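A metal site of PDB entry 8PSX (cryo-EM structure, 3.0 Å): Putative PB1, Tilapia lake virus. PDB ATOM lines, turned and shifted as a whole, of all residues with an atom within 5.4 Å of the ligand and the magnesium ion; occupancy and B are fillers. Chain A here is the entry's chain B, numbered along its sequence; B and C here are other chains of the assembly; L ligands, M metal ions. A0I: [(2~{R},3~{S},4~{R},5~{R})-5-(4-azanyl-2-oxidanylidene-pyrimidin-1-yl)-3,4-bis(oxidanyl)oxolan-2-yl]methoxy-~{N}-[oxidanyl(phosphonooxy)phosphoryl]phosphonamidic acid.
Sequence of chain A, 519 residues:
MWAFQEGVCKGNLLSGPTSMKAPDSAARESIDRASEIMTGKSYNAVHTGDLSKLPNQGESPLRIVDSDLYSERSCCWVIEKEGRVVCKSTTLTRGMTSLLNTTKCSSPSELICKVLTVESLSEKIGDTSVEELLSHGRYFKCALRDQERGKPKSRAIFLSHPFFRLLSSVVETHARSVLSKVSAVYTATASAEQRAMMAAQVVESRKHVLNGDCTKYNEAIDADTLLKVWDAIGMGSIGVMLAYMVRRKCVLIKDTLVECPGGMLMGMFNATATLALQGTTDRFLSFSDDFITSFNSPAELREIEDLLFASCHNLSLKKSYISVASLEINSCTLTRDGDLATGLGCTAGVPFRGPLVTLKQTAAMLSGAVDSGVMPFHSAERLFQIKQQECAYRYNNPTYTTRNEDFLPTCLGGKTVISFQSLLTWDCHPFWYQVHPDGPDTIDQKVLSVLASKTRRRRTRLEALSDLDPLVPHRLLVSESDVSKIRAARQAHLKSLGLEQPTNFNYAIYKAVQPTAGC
Residues that only touch the ligand: Met 266 (3.7 Å) and U 31 of chain B (3.7 Å).
Hydrophobic or aromatic side chains that line the ligand: Tyr 217 and Met 266.
The backbone carbonyl oxygen (O) of Asp 213 sits at hydrogen-bond distance from the backbone NH (N) of Ser 316 (2.7 Å).
The side-chain carboxylate (OD1) of Asp 289 sits close to O3' of A 21 of chain C (2.7 Å).
The side-chain carboxylate (OE2) of Glu 148 lies within salt-bridge range of the guanidinium group (NE) of Arg 155 (2.5 Å).
SD of Met 266 lies within hydrogen-bond range of NH1 of Arg 155, 3.3 Å away.
O6 of G 30 of chain B sits at hydrogen-bond distance from the guanidinium group (NE) of Arg 145, 2.8 Å away.
The side-chain amide oxygen (OD1) of Asn 218 lies within hydrogen-bond range of the backbone NH (N) of Met 266 (3.2 Å).
ND2 of Asn 218 sits at hydrogen-bond distance from OE1 of Glu 219 (2.7 Å).
O2' of A 21 of chain C lies within hydrogen-bond range of the side-chain hydroxyl (OG) of Ser 288 (3.3 Å).
Of the 22 residues printed, 3 come within 4 Å of the magnesium ion.
Along chain A the residues within 4 Å of the magnesium ion span positions 213 to 289.
The nearest printed residue that does not touch the magnesium ion is Thr 215 (4.5 Å).
An oxygen (O11) of the ligand is in salt-bridge range of the guanidinium group of Arg 155, 2.7 Å away.
O6 of G 30 of chain B is in hydrogen-bond range of N3 of the ligand, at 3.3 Å.
An oxygen (O12) of the ligand sits at hydrogen-bond distance from the side-chain amide nitrogen of Asn 218 (2.8 Å).
N of Gly 267 is in hydrogen-bond range of O13 of the ligand (3.2 Å).
N6 of A 21 of chain C is in hydrogen-bond range of a nitrogen (N3) of the ligand.
O9 of the ligand is in hydrogen-bond range of OG1 of Thr 215.
The backbone NH of Lys 216 sits at hydrogen-bond distance from an oxygen (O5) of the ligand (3.4 Å).
The side-chain carboxylate (OE1) of Glu 148 sits at hydrogen-bond distance from a nitrogen (N3) of the ligand (3.4 Å).
The backbone NH (N) of Tyr 217 is in hydrogen-bond range of an oxygen (O5) of the ligand, at 3.4 Å.
O11 of the ligand lies within salt-bridge range of NZ of Lys 151, 3.8 Å away.
The magnesium ion is bound by an oxygen (O8) of the ligand (1.9 Å), an oxygen (O4) of the ligand (2.2 Å), the side-chain carboxylate of Asp 213 (2.3 Å), the backbone carbonyl oxygen of Cys 214 (2.4 Å) and the side-chain carboxylate of Asp 289 (2.5 Å).
The magnesium ion has five donor atoms within binding distance.
Slightly farther from the magnesium ion lies O6 of the ligand (2.6 Å).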
ATOM      1  N   ARG A 145     -21.932 -17.646 -14.303  1.00  0.00           N
ATOM      2  CA  ARG A 145     -21.196 -18.488 -15.235  1.00  0.00           C
ATOM      3  C   ARG A 145     -22.207 -19.187 -16.127  1.00  0.00           C
ATOM      4  O   ARG A 145     -23.085 -19.909 -15.636  1.00  0.00           O
ATOM      5  CB  ARG A 145     -20.318 -19.493 -14.493  1.00  0.00           C
ATOM      6  CG  ARG A 145     -19.636 -20.530 -15.380  1.00  0.00           C
ATOM      7  CD  ARG A 145     -18.283 -20.055 -15.878  1.00  0.00           C
ATOM      8  NE  ARG A 145     -17.311 -21.135 -15.922  1.00  0.00           N
ATOM      9  CZ  ARG A 145     -17.200 -22.014 -16.913  1.00  0.00           C
ATOM     10  NH1 ARG A 145     -18.003 -21.966 -17.963  1.00  0.00           N
ATOM     11  NH2 ARG A 145     -16.275 -22.965 -16.846  1.00  0.00           N
ATOM     12  N   GLU A 148     -22.383 -23.408 -20.066  1.00  0.00           N
ATOM     13  CA  GLU A 148     -22.227 -24.775 -19.567  1.00  0.00           C
ATOM     14  C   GLU A 148     -23.341 -25.633 -20.147  1.00  0.00           C
ATOM     15  O   GLU A 148     -24.521 -25.393 -19.858  1.00  0.00           O
ATOM     16  CB  GLU A 148     -22.255 -24.810 -18.042  1.00  0.00           C
ATOM     17  CG  GLU A 148     -21.059 -24.164 -17.376  1.00  0.00           C
ATOM     18  CD  GLU A 148     -20.830 -24.665 -15.968  1.00  0.00           C
ATOM     19  OE1 GLU A 148     -20.153 -25.701 -15.799  1.00  0.00           O
ATOM     20  OE2 GLU A 148     -21.339 -24.032 -15.022  1.00  0.00           O
ATOM     21  N   LYS A 151     -27.149 -26.984 -18.660  1.00  0.00           N
ATOM     22  CA  LYS A 151     -27.532 -26.124 -17.541  1.00  0.00           C
ATOM     23  C   LYS A 151     -28.239 -24.892 -18.085  1.00  0.00           C
ATOM     24  O   LYS A 151     -27.633 -23.827 -18.228  1.00  0.00           O
ATOM     25  CB  LYS A 151     -26.319 -25.730 -16.707  1.00  0.00           C
ATOM     26  CG  LYS A 151     -25.727 -26.873 -15.902  1.00  0.00           C
ATOM     27  CD  LYS A 151     -24.934 -26.372 -14.711  1.00  0.00           C
ATOM     28  CE  LYS A 151     -25.846 -25.958 -13.564  1.00  0.00           C
ATOM     29  NZ  LYS A 151     -25.782 -26.901 -12.423  1.00  0.00           N
ATOM     30  N   ARG A 155     -24.996 -20.915 -13.604  1.00  0.00           N
ATOM     31  CA  ARG A 155     -24.648 -21.073 -12.196  1.00  0.00           C
ATOM     32  C   ARG A 155     -24.070 -19.772 -11.635  1.00  0.00           C
ATOM     33  O   ARG A 155     -23.639 -18.884 -12.369  1.00  0.00           O
ATOM     34  CB  ARG A 155     -23.668 -22.231 -12.012  1.00  0.00           C
ATOM     35  CG  ARG A 155     -22.210 -21.904 -12.294  1.00  0.00           C
ATOM     36  CD  ARG A 155     -21.295 -23.062 -11.929  1.00  0.00           C
ATOM     37  NE  ARG A 155     -21.669 -24.300 -12.603  1.00  0.00           N
ATOM     38  CZ  ARG A 155     -21.968 -25.435 -11.992  1.00  0.00           C
ATOM     39  NH1 ARG A 155     -21.967 -25.543 -10.673  1.00  0.00           N
ATOM     40  NH2 ARG A 155     -22.274 -26.502 -12.724  1.00  0.00           N
ATOM     41  N   ASP A 213     -22.812 -39.353  -8.284  1.00  0.00           N
ATOM     42  CA  ASP A 213     -22.669 -37.903  -8.265  1.00  0.00           C
ATOM     43  C   ASP A 213     -23.309 -37.383  -6.980  1.00  0.00           C
ATOM     44  O   ASP A 213     -24.142 -38.066  -6.367  1.00  0.00           O
ATOM     45  CB  ASP A 213     -23.326 -37.248  -9.495  1.00  0.00           C
ATOM     46  CG  ASP A 213     -22.791 -35.851  -9.762  1.00  0.00           C
ATOM     47  OD1 ASP A 213     -21.603 -35.723 -10.114  1.00  0.00           O
ATOM     48  OD2 ASP A 213     -23.565 -34.883  -9.613  1.00  0.00           O
ATOM     49  N   CYS A 214     -22.910 -36.186  -6.575  1.00  0.00           N
ATOM     50  CA  CYS A 214     -23.440 -35.564  -5.365  1.00  0.00           C
ATOM     51  C   CYS A 214     -24.169 -34.279  -5.744  1.00  0.00           C
ATOM     52  O   CYS A 214     -23.812 -33.597  -6.715  1.00  0.00           O
ATOM     53  CB  CYS A 214     -22.346 -35.251  -4.349  1.00  0.00           C
ATOM     54  SG  CYS A 214     -21.291 -36.662  -3.933  1.00  0.00           S
ATOM     55  N   THR A 215     -25.196 -33.957  -4.968  1.00  0.00           N
ATOM     56  CA  THR A 215     -26.032 -32.797  -5.200  1.00  0.00           C
ATOM     57  C   THR A 215     -25.811 -31.771  -4.101  1.00  0.00           C
ATOM     58  O   THR A 215     -25.590 -32.124  -2.938  1.00  0.00           O
ATOM     59  CB  THR A 215     -27.515 -33.194  -5.257  1.00  0.00           C
ATOM     60  OG1 THR A 215     -28.312 -32.050  -5.568  1.00  0.00           O
ATOM     61  CG2 THR A 215     -27.971 -33.802  -3.934  1.00  0.00           C
ATOM     62  N   LYS A 216     -25.862 -30.489  -4.467  1.00  0.00           N
ATOM     63  CA  LYS A 216     -25.617 -29.394  -3.532  1.00  0.00           C
ATOM     64  C   LYS A 216     -24.278 -29.583  -2.830  1.00  0.00           C
ATOM     65  O   LYS A 216     -24.154 -29.387  -1.619  1.00  0.00           O
ATOM     66  CB  LYS A 216     -26.759 -29.268  -2.517  1.00  0.00           C
ATOM     67  CG  LYS A 216     -28.158 -29.366  -3.112  1.00  0.00           C
ATOM     68  CD  LYS A 216     -28.569 -28.067  -3.787  1.00  0.00           C
ATOM     69  CE  LYS A 216     -29.385 -28.329  -5.034  1.00  0.00           C
ATOM     70  NZ  LYS A 216     -30.590 -29.175  -4.754  1.00  0.00           N
ATOM     71  N   TYR A 217     -23.270 -29.972  -3.598  1.00  0.00           N
ATOM     72  CA  TYR A 217     -21.980 -30.333  -3.021  1.00  0.00           C
ATOM     73  C   TYR A 217     -21.393 -29.191  -2.202  1.00  0.00           C
ATOM     74  O   TYR A 217     -21.024 -29.379  -1.031  1.00  0.00           O
ATOM     75  CB  TYR A 217     -21.009 -30.739  -4.127  1.00  0.00           C
ATOM     76  CG  TYR A 217     -19.705 -31.314  -3.615  1.00  0.00           C
ATOM     77  CD1 TYR A 217     -19.678 -32.526  -2.948  1.00  0.00           C
ATOM     78  CD2 TYR A 217     -18.505 -30.642  -3.803  1.00  0.00           C
ATOM     79  CE1 TYR A 217     -18.495 -33.056  -2.494  1.00  0.00           C
ATOM     80  CE2 TYR A 217     -17.324 -31.162  -3.340  1.00  0.00           C
ATOM     81  CZ  TYR A 217     -17.315 -32.370  -2.683  1.00  0.00           C
ATOM     82  OH  TYR A 217     -16.137 -32.899  -2.220  1.00  0.00           O
ATOM     83  N   ASN A 218     -21.308 -28.003  -2.784  1.00  0.00           N
ATOM     84  CA  ASN A 218     -20.663 -26.891  -2.101  1.00  0.00           C
ATOM     85  C   ASN A 218     -21.531 -26.353  -0.964  1.00  0.00           C
ATOM     86  O   ASN A 218     -21.005 -25.773  -0.015  1.00  0.00           O
ATOM     87  CB  ASN A 218     -20.332 -25.774  -3.091  1.00  0.00           C
ATOM     88  CG  ASN A 218     -21.563 -25.090  -3.630  1.00  0.00           C
ATOM     89  OD1 ASN A 218     -22.088 -24.161  -3.026  1.00  0.00           O
ATOM     90  ND2 ASN A 218     -22.029 -25.546  -4.786  1.00  0.00           N
ATOM     91  N   GLU A 219     -22.853 -26.526  -1.056  1.00  0.00           N
ATOM     92  CA  GLU A 219     -23.736 -26.055   0.000  1.00  0.00           C
ATOM     93  C   GLU A 219     -23.710 -26.962   1.220  1.00  0.00           C
ATOM     94  O   GLU A 219     -23.966 -26.494   2.340  1.00  0.00           O
ATOM     95  CB  GLU A 219     -25.166 -25.923  -0.518  1.00  0.00           C
ATOM     96  CG  GLU A 219     -25.345 -24.807  -1.531  1.00  0.00           C
ATOM     97  CD  GLU A 219     -25.504 -25.328  -2.949  1.00  0.00           C
ATOM     98  OE1 GLU A 219     -24.466 -25.501  -3.628  1.00  0.00           O
ATOM     99  OE2 GLU A 219     -26.638 -25.553  -3.379  1.00  0.00           O
ATOM    100  N   MET A 264     -19.662 -23.577   1.267  1.00  0.00           N
ATOM    101  CA  MET A 264     -18.318 -23.085   1.001  1.00  0.00           C
ATOM    102  C   MET A 264     -18.242 -22.269  -0.293  1.00  0.00           C
ATOM    103  O   MET A 264     -17.147 -21.988  -0.776  1.00  0.00           O
ATOM    104  CB  MET A 264     -17.322 -24.251   0.944  1.00  0.00           C
ATOM    105  CG  MET A 264     -17.580 -25.259  -0.166  1.00  0.00           C
ATOM    106  SD  MET A 264     -16.184 -26.378  -0.400  1.00  0.00           S
ATOM    107  CE  MET A 264     -16.626 -27.126  -1.961  1.00  0.00           C
ATOM    108  N   MET A 266     -19.331 -22.678  -3.700  1.00  0.00           N
ATOM    109  CA  MET A 266     -19.119 -23.182  -5.068  1.00  0.00           C
ATOM    110  C   MET A 266     -17.639 -23.451  -5.342  1.00  0.00           C
ATOM    111  O   MET A 266     -16.959 -22.736  -6.087  1.00  0.00           O
ATOM    112  CB  MET A 266     -19.719 -22.206  -6.090  1.00  0.00           C
ATOM    113  CG  MET A 266     -19.475 -22.593  -7.554  1.00  0.00           C
ATOM    114  SD  MET A 266     -20.704 -23.711  -8.276  1.00  0.00           S
ATOM    115  CE  MET A 266     -22.262 -22.887  -7.966  1.00  0.00           C
ATOM    116  N   GLY A 267     -17.145 -24.491  -4.679  1.00  0.00           N
ATOM    117  CA  GLY A 267     -15.853 -25.057  -5.040  1.00  0.00           C
ATOM    118  C   GLY A 267     -14.661 -24.243  -4.595  1.00  0.00           C
ATOM    119  O   GLY A 267     -13.652 -24.205  -5.309  1.00  0.00           O
ATOM    120  N   ASN A 270     -11.872 -27.632  -3.131  1.00  0.00           N
ATOM    121  CA  ASN A 270     -12.129 -28.935  -3.748  1.00  0.00           C
ATOM    122  C   ASN A 270     -11.307 -30.029  -3.086  1.00  0.00           C
ATOM    123  O   ASN A 270     -11.808 -31.118  -2.827  1.00  0.00           O
ATOM    124  CB  ASN A 270     -11.848 -28.869  -5.254  1.00  0.00           C
ATOM    125  CG  ASN A 270     -12.743 -27.881  -5.969  1.00  0.00           C
ATOM    126  OD1 ASN A 270     -13.958 -27.907  -5.823  1.00  0.00           O
ATOM    127  ND2 ASN A 270     -12.139 -27.007  -6.768  1.00  0.00           N
ATOM    128  N   SER A 288     -13.696 -34.233  -5.756  1.00  0.00           N
ATOM    129  CA  SER A 288     -14.844 -33.322  -5.690  1.00  0.00           C
ATOM    130  C   SER A 288     -16.110 -34.192  -5.668  1.00  0.00           C
ATOM    131  O   SER A 288     -16.140 -35.200  -4.947  1.00  0.00           O
ATOM    132  CB  SER A 288     -14.769 -32.325  -6.830  1.00  0.00           C
ATOM    133  OG  SER A 288     -15.771 -31.333  -6.703  1.00  0.00           O
ATOM    134  N   ASP A 289     -17.144 -33.859  -6.423  1.00  0.00           N
ATOM    135  CA  ASP A 289     -18.418 -34.586  -6.373  1.00  0.00           C
ATOM    136  C   ASP A 289     -18.532 -35.570  -7.544  1.00  0.00           C
ATOM    137  O   ASP A 289     -19.444 -35.504  -8.369  1.00  0.00           O
ATOM    138  CB  ASP A 289     -19.579 -33.590  -6.355  1.00  0.00           C
ATOM    139  CG  ASP A 289     -19.920 -33.046  -7.713  1.00  0.00           C
ATOM    140  OD1 ASP A 289     -18.995 -32.878  -8.539  1.00  0.00           O
ATOM    141  OD2 ASP A 289     -21.117 -32.803  -7.978  1.00  0.00           O
ATOM    142  N   SER A 316     -26.587 -37.999  -5.227  1.00  0.00           N
ATOM    143  CA  SER A 316     -27.552 -37.341  -6.110  1.00  0.00           C
ATOM    144  C   SER A 316     -28.453 -38.414  -6.694  1.00  0.00           C
ATOM    145  O   SER A 316     -28.072 -39.135  -7.611  1.00  0.00           O
ATOM    146  CB  SER A 316     -26.832 -36.555  -7.192  1.00  0.00           C
ATOM    147  OG  SER A 316     -27.747 -36.098  -8.179  1.00  0.00           O
ATOM    148  N   LYS A 319     -29.143 -38.240 -10.621  1.00  0.00           N
ATOM    149  CA  LYS A 319     -28.121 -38.577 -11.603  1.00  0.00           C
ATOM    150  C   LYS A 319     -27.372 -39.864 -11.304  1.00  0.00           C
ATOM    151  O   LYS A 319     -26.908 -40.519 -12.239  1.00  0.00           O
ATOM    152  CB  LYS A 319     -27.110 -37.440 -11.716  1.00  0.00           C
ATOM    153  CG  LYS A 319     -27.734 -36.087 -11.987  1.00  0.00           C
ATOM    154  CD  LYS A 319     -26.697 -35.061 -12.396  1.00  0.00           C
ATOM    155  CE  LYS A 319     -27.348 -33.760 -12.848  1.00  0.00           C
ATOM    156  NZ  LYS A 319     -26.362 -32.813 -13.426  1.00  0.00           N
ATOM    157  P     G B  30     -13.131 -14.898 -13.947  1.00  0.00           P
ATOM    158  OP1   G B  30     -12.458 -13.591 -14.098  1.00  0.00           O
ATOM    159  OP2   G B  30     -13.002 -15.923 -15.007  1.00  0.00           O
ATOM    160  O5'   G B  30     -12.633 -15.545 -12.576  1.00  0.00           O
ATOM    161  C5'   G B  30     -12.630 -14.794 -11.376  1.00  0.00           C
ATOM    162  C4'   G B  30     -13.095 -15.612 -10.199  1.00  0.00           C
ATOM    163  O4'   G B  30     -14.478 -16.006 -10.373  1.00  0.00           O
ATOM    164  C3'   G B  30     -12.357 -16.926  -9.973  1.00  0.00           C
ATOM    165  O3'   G B  30     -11.126 -16.766  -9.303  1.00  0.00           O
ATOM    166  C2'   G B  30     -13.382 -17.737  -9.189  1.00  0.00           C
ATOM    167  O2'   G B  30     -13.390 -17.375  -7.824  1.00  0.00           O
ATOM    168  C1'   G B  30     -14.685 -17.291  -9.837  1.00  0.00           C
ATOM    169  N9    G B  30     -15.117 -18.183 -10.925  1.00  0.00           N
ATOM    170  C8    G B  30     -15.234 -17.858 -12.245  1.00  0.00           C
ATOM    171  N7    G B  30     -15.650 -18.862 -12.985  1.00  0.00           N
ATOM    172  C5    G B  30     -15.803 -19.900 -12.077  1.00  0.00           C
ATOM    173  C6    G B  30     -16.225 -21.229 -12.280  1.00  0.00           C
ATOM    174  O6    G B  30     -16.555 -21.785 -13.342  1.00  0.00           O
ATOM    175  N1    G B  30     -16.243 -21.953 -11.099  1.00  0.00           N
ATOM    176  C2    G B  30     -15.903 -21.454  -9.867  1.00  0.00           C
ATOM    177  N2    G B  30     -15.983 -22.314  -8.855  1.00  0.00           N
ATOM    178  N3    G B  30     -15.503 -20.212  -9.657  1.00  0.00           N
ATOM    179  C4    G B  30     -15.484 -19.499 -10.803  1.00  0.00           C
ATOM    180  P     U B  31      -9.901 -17.748  -9.618  1.00  0.00           P
ATOM    181  OP1   U B  31      -8.691 -17.176  -8.983  1.00  0.00           O
ATOM    182  OP2   U B  31      -9.894 -18.058 -11.067  1.00  0.00           O
ATOM    183  O5'   U B  31     -10.284 -19.095  -8.852  1.00  0.00           O
ATOM    184  C5'   U B  31     -10.422 -19.126  -7.443  1.00  0.00           C
ATOM    185  C4'   U B  31     -10.735 -20.521  -6.966  1.00  0.00           C
ATOM    186  O4'   U B  31     -12.081 -20.887  -7.384  1.00  0.00           O
ATOM    187  C3'   U B  31      -9.859 -21.622  -7.538  1.00  0.00           C
ATOM    188  O3'   U B  31      -8.616 -21.750  -6.871  1.00  0.00           O
ATOM    189  C2'   U B  31     -10.741 -22.846  -7.438  1.00  0.00           C
ATOM    190  O2'   U B  31     -10.735 -23.383  -6.124  1.00  0.00           O
ATOM    191  C1'   U B  31     -12.124 -22.259  -7.720  1.00  0.00           C
ATOM    192  N1    U B  31     -12.493 -22.371  -9.150  1.00  0.00           N
ATOM    193  C2    U B  31     -12.980 -23.581  -9.591  1.00  0.00           C
ATOM    194  O2    U B  31     -13.094 -24.552  -8.873  1.00  0.00           O
ATOM    195  N3    U B  31     -13.313 -23.611 -10.928  1.00  0.00           N
ATOM    196  C4    U B  31     -13.221 -22.581 -11.834  1.00  0.00           C
ATOM    197  O4    U B  31     -13.560 -22.766 -12.990  1.00  0.00           O
ATOM    198  C5    U B  31     -12.717 -21.356 -11.294  1.00  0.00           C
ATOM    199  C6    U B  31     -12.376 -21.297 -10.001  1.00  0.00           C
ATOM    200  P     A C  21     -18.126 -33.359 -16.126  1.00  0.00           P
ATOM    201  OP1   A C  21     -18.984 -34.550 -15.891  1.00  0.00           O
ATOM    202  OP2   A C  21     -18.642 -32.221 -16.923  1.00  0.00           O
ATOM    203  O5'   A C  21     -17.666 -32.796 -14.710  1.00  0.00           O
ATOM    204  C5'   A C  21     -17.158 -33.661 -13.712  1.00  0.00           C
ATOM    205  C4'   A C  21     -16.841 -32.924 -12.433  1.00  0.00           C
ATOM    206  O4'   A C  21     -15.691 -32.068 -12.630  1.00  0.00           O
ATOM    207  C3'   A C  21     -17.917 -31.985 -11.921  1.00  0.00           C
ATOM    208  O3'   A C  21     -18.952 -32.659 -11.234  1.00  0.00           O
ATOM    209  C2'   A C  21     -17.119 -31.030 -11.029  1.00  0.00           C
ATOM    210  O2'   A C  21     -16.877 -31.603  -9.755  1.00  0.00           O
ATOM    211  C1'   A C  21     -15.790 -30.932 -11.792  1.00  0.00           C
ATOM    212  N9    A C  21     -15.700 -29.711 -12.601  1.00  0.00           N
ATOM    213  C8    A C  21     -16.060 -29.501 -13.906  1.00  0.00           C
ATOM    214  N7    A C  21     -15.849 -28.270 -14.321  1.00  0.00           N
ATOM    215  C5    A C  21     -15.310 -27.635 -13.210  1.00  0.00           C
ATOM    216  C6    A C  21     -14.881 -26.317 -12.981  1.00  0.00           C
ATOM    217  N6    A C  21     -14.891 -25.339 -13.891  1.00  0.00           N
ATOM    218  N1    A C  21     -14.408 -26.018 -11.751  1.00  0.00           N
ATOM    219  C2    A C  21     -14.382 -26.979 -10.822  1.00  0.00           C
ATOM    220  N3    A C  21     -14.769 -28.247 -10.919  1.00  0.00           N
ATOM    221  C4    A C  21     -15.225 -28.509 -12.144  1.00  0.00           C
HETATM  222  C1  A0I L   1     -18.744 -26.617 -12.024  1.00  0.00           C
HETATM  223  C2  A0I L   1     -18.636 -27.264 -10.851  1.00  0.00           C
HETATM  224  C3  A0I L   1     -17.331 -25.482  -9.930  1.00  0.00           C
HETATM  225  C4  A0I L   1     -18.116 -25.343 -12.128  1.00  0.00           C
HETATM  226  C5  A0I L   1     -17.814 -27.443  -8.504  1.00  0.00           C
HETATM  227  C6  A0I L   1     -18.673 -26.815  -7.392  1.00  0.00           C
HETATM  228  C7  A0I L   1     -19.995 -27.557  -7.616  1.00  0.00           C
HETATM  229  C8  A0I L   1     -19.470 -28.972  -7.883  1.00  0.00           C
HETATM  230  C9  A0I L   1     -20.452 -29.916  -8.544  1.00  0.00           C
HETATM  231  N1  A0I L   1     -17.951 -26.737  -9.812  1.00  0.00           N
HETATM  232  N2  A0I L   1     -17.435 -24.816 -11.103  1.00  0.00           N
HETATM  233  N3  A0I L   1     -18.183 -24.645 -13.250  1.00  0.00           N
HETATM  234  N4  A0I L   1     -23.407 -28.860  -8.960  1.00  0.00           N
HETATM  235  O1  A0I L   1     -16.719 -25.032  -8.957  1.00  0.00           O
HETATM  236  O10 A0I L   1     -25.856 -30.241 -10.350  1.00  0.00           O
HETATM  237  O11 A0I L   1     -22.699 -28.819 -11.453  1.00  0.00           O
HETATM  238  O12 A0I L   1     -20.881 -27.504  -6.503  1.00  0.00           O
HETATM  239  O13 A0I L   1     -18.093 -27.118  -6.143  1.00  0.00           O
HETATM  240  O2  A0I L   1     -18.291 -28.762  -8.690  1.00  0.00           O
HETATM  241  O3  A0I L   1     -21.020 -29.290  -9.713  1.00  0.00           O
HETATM  242  O4  A0I L   1     -22.684 -31.050 -10.168  1.00  0.00           O
HETATM  243  O5  A0I L   1     -24.165 -28.410  -6.526  1.00  0.00           O
HETATM  244  O6  A0I L   1     -23.234 -30.736  -7.133  1.00  0.00           O
HETATM  245  O7  A0I L   1     -25.432 -29.967  -7.891  1.00  0.00           O
HETATM  246  O8  A0I L   1     -25.281 -32.251  -8.920  1.00  0.00           O
HETATM  247  O9  A0I L   1     -27.508 -31.108  -8.668  1.00  0.00           O
HETATM  248  P1  A0I L   1     -22.528 -29.562 -10.158  1.00  0.00           P
HETATM  249  P2  A0I L   1     -23.942 -29.485  -7.542  1.00  0.00           P
HETATM  250  P3  A0I L   1     -26.044 -30.944  -9.023  1.00  0.00           P
HETATM  251 MG    MG M   1     -23.430 -32.702  -8.865  1.00  0.00          MG
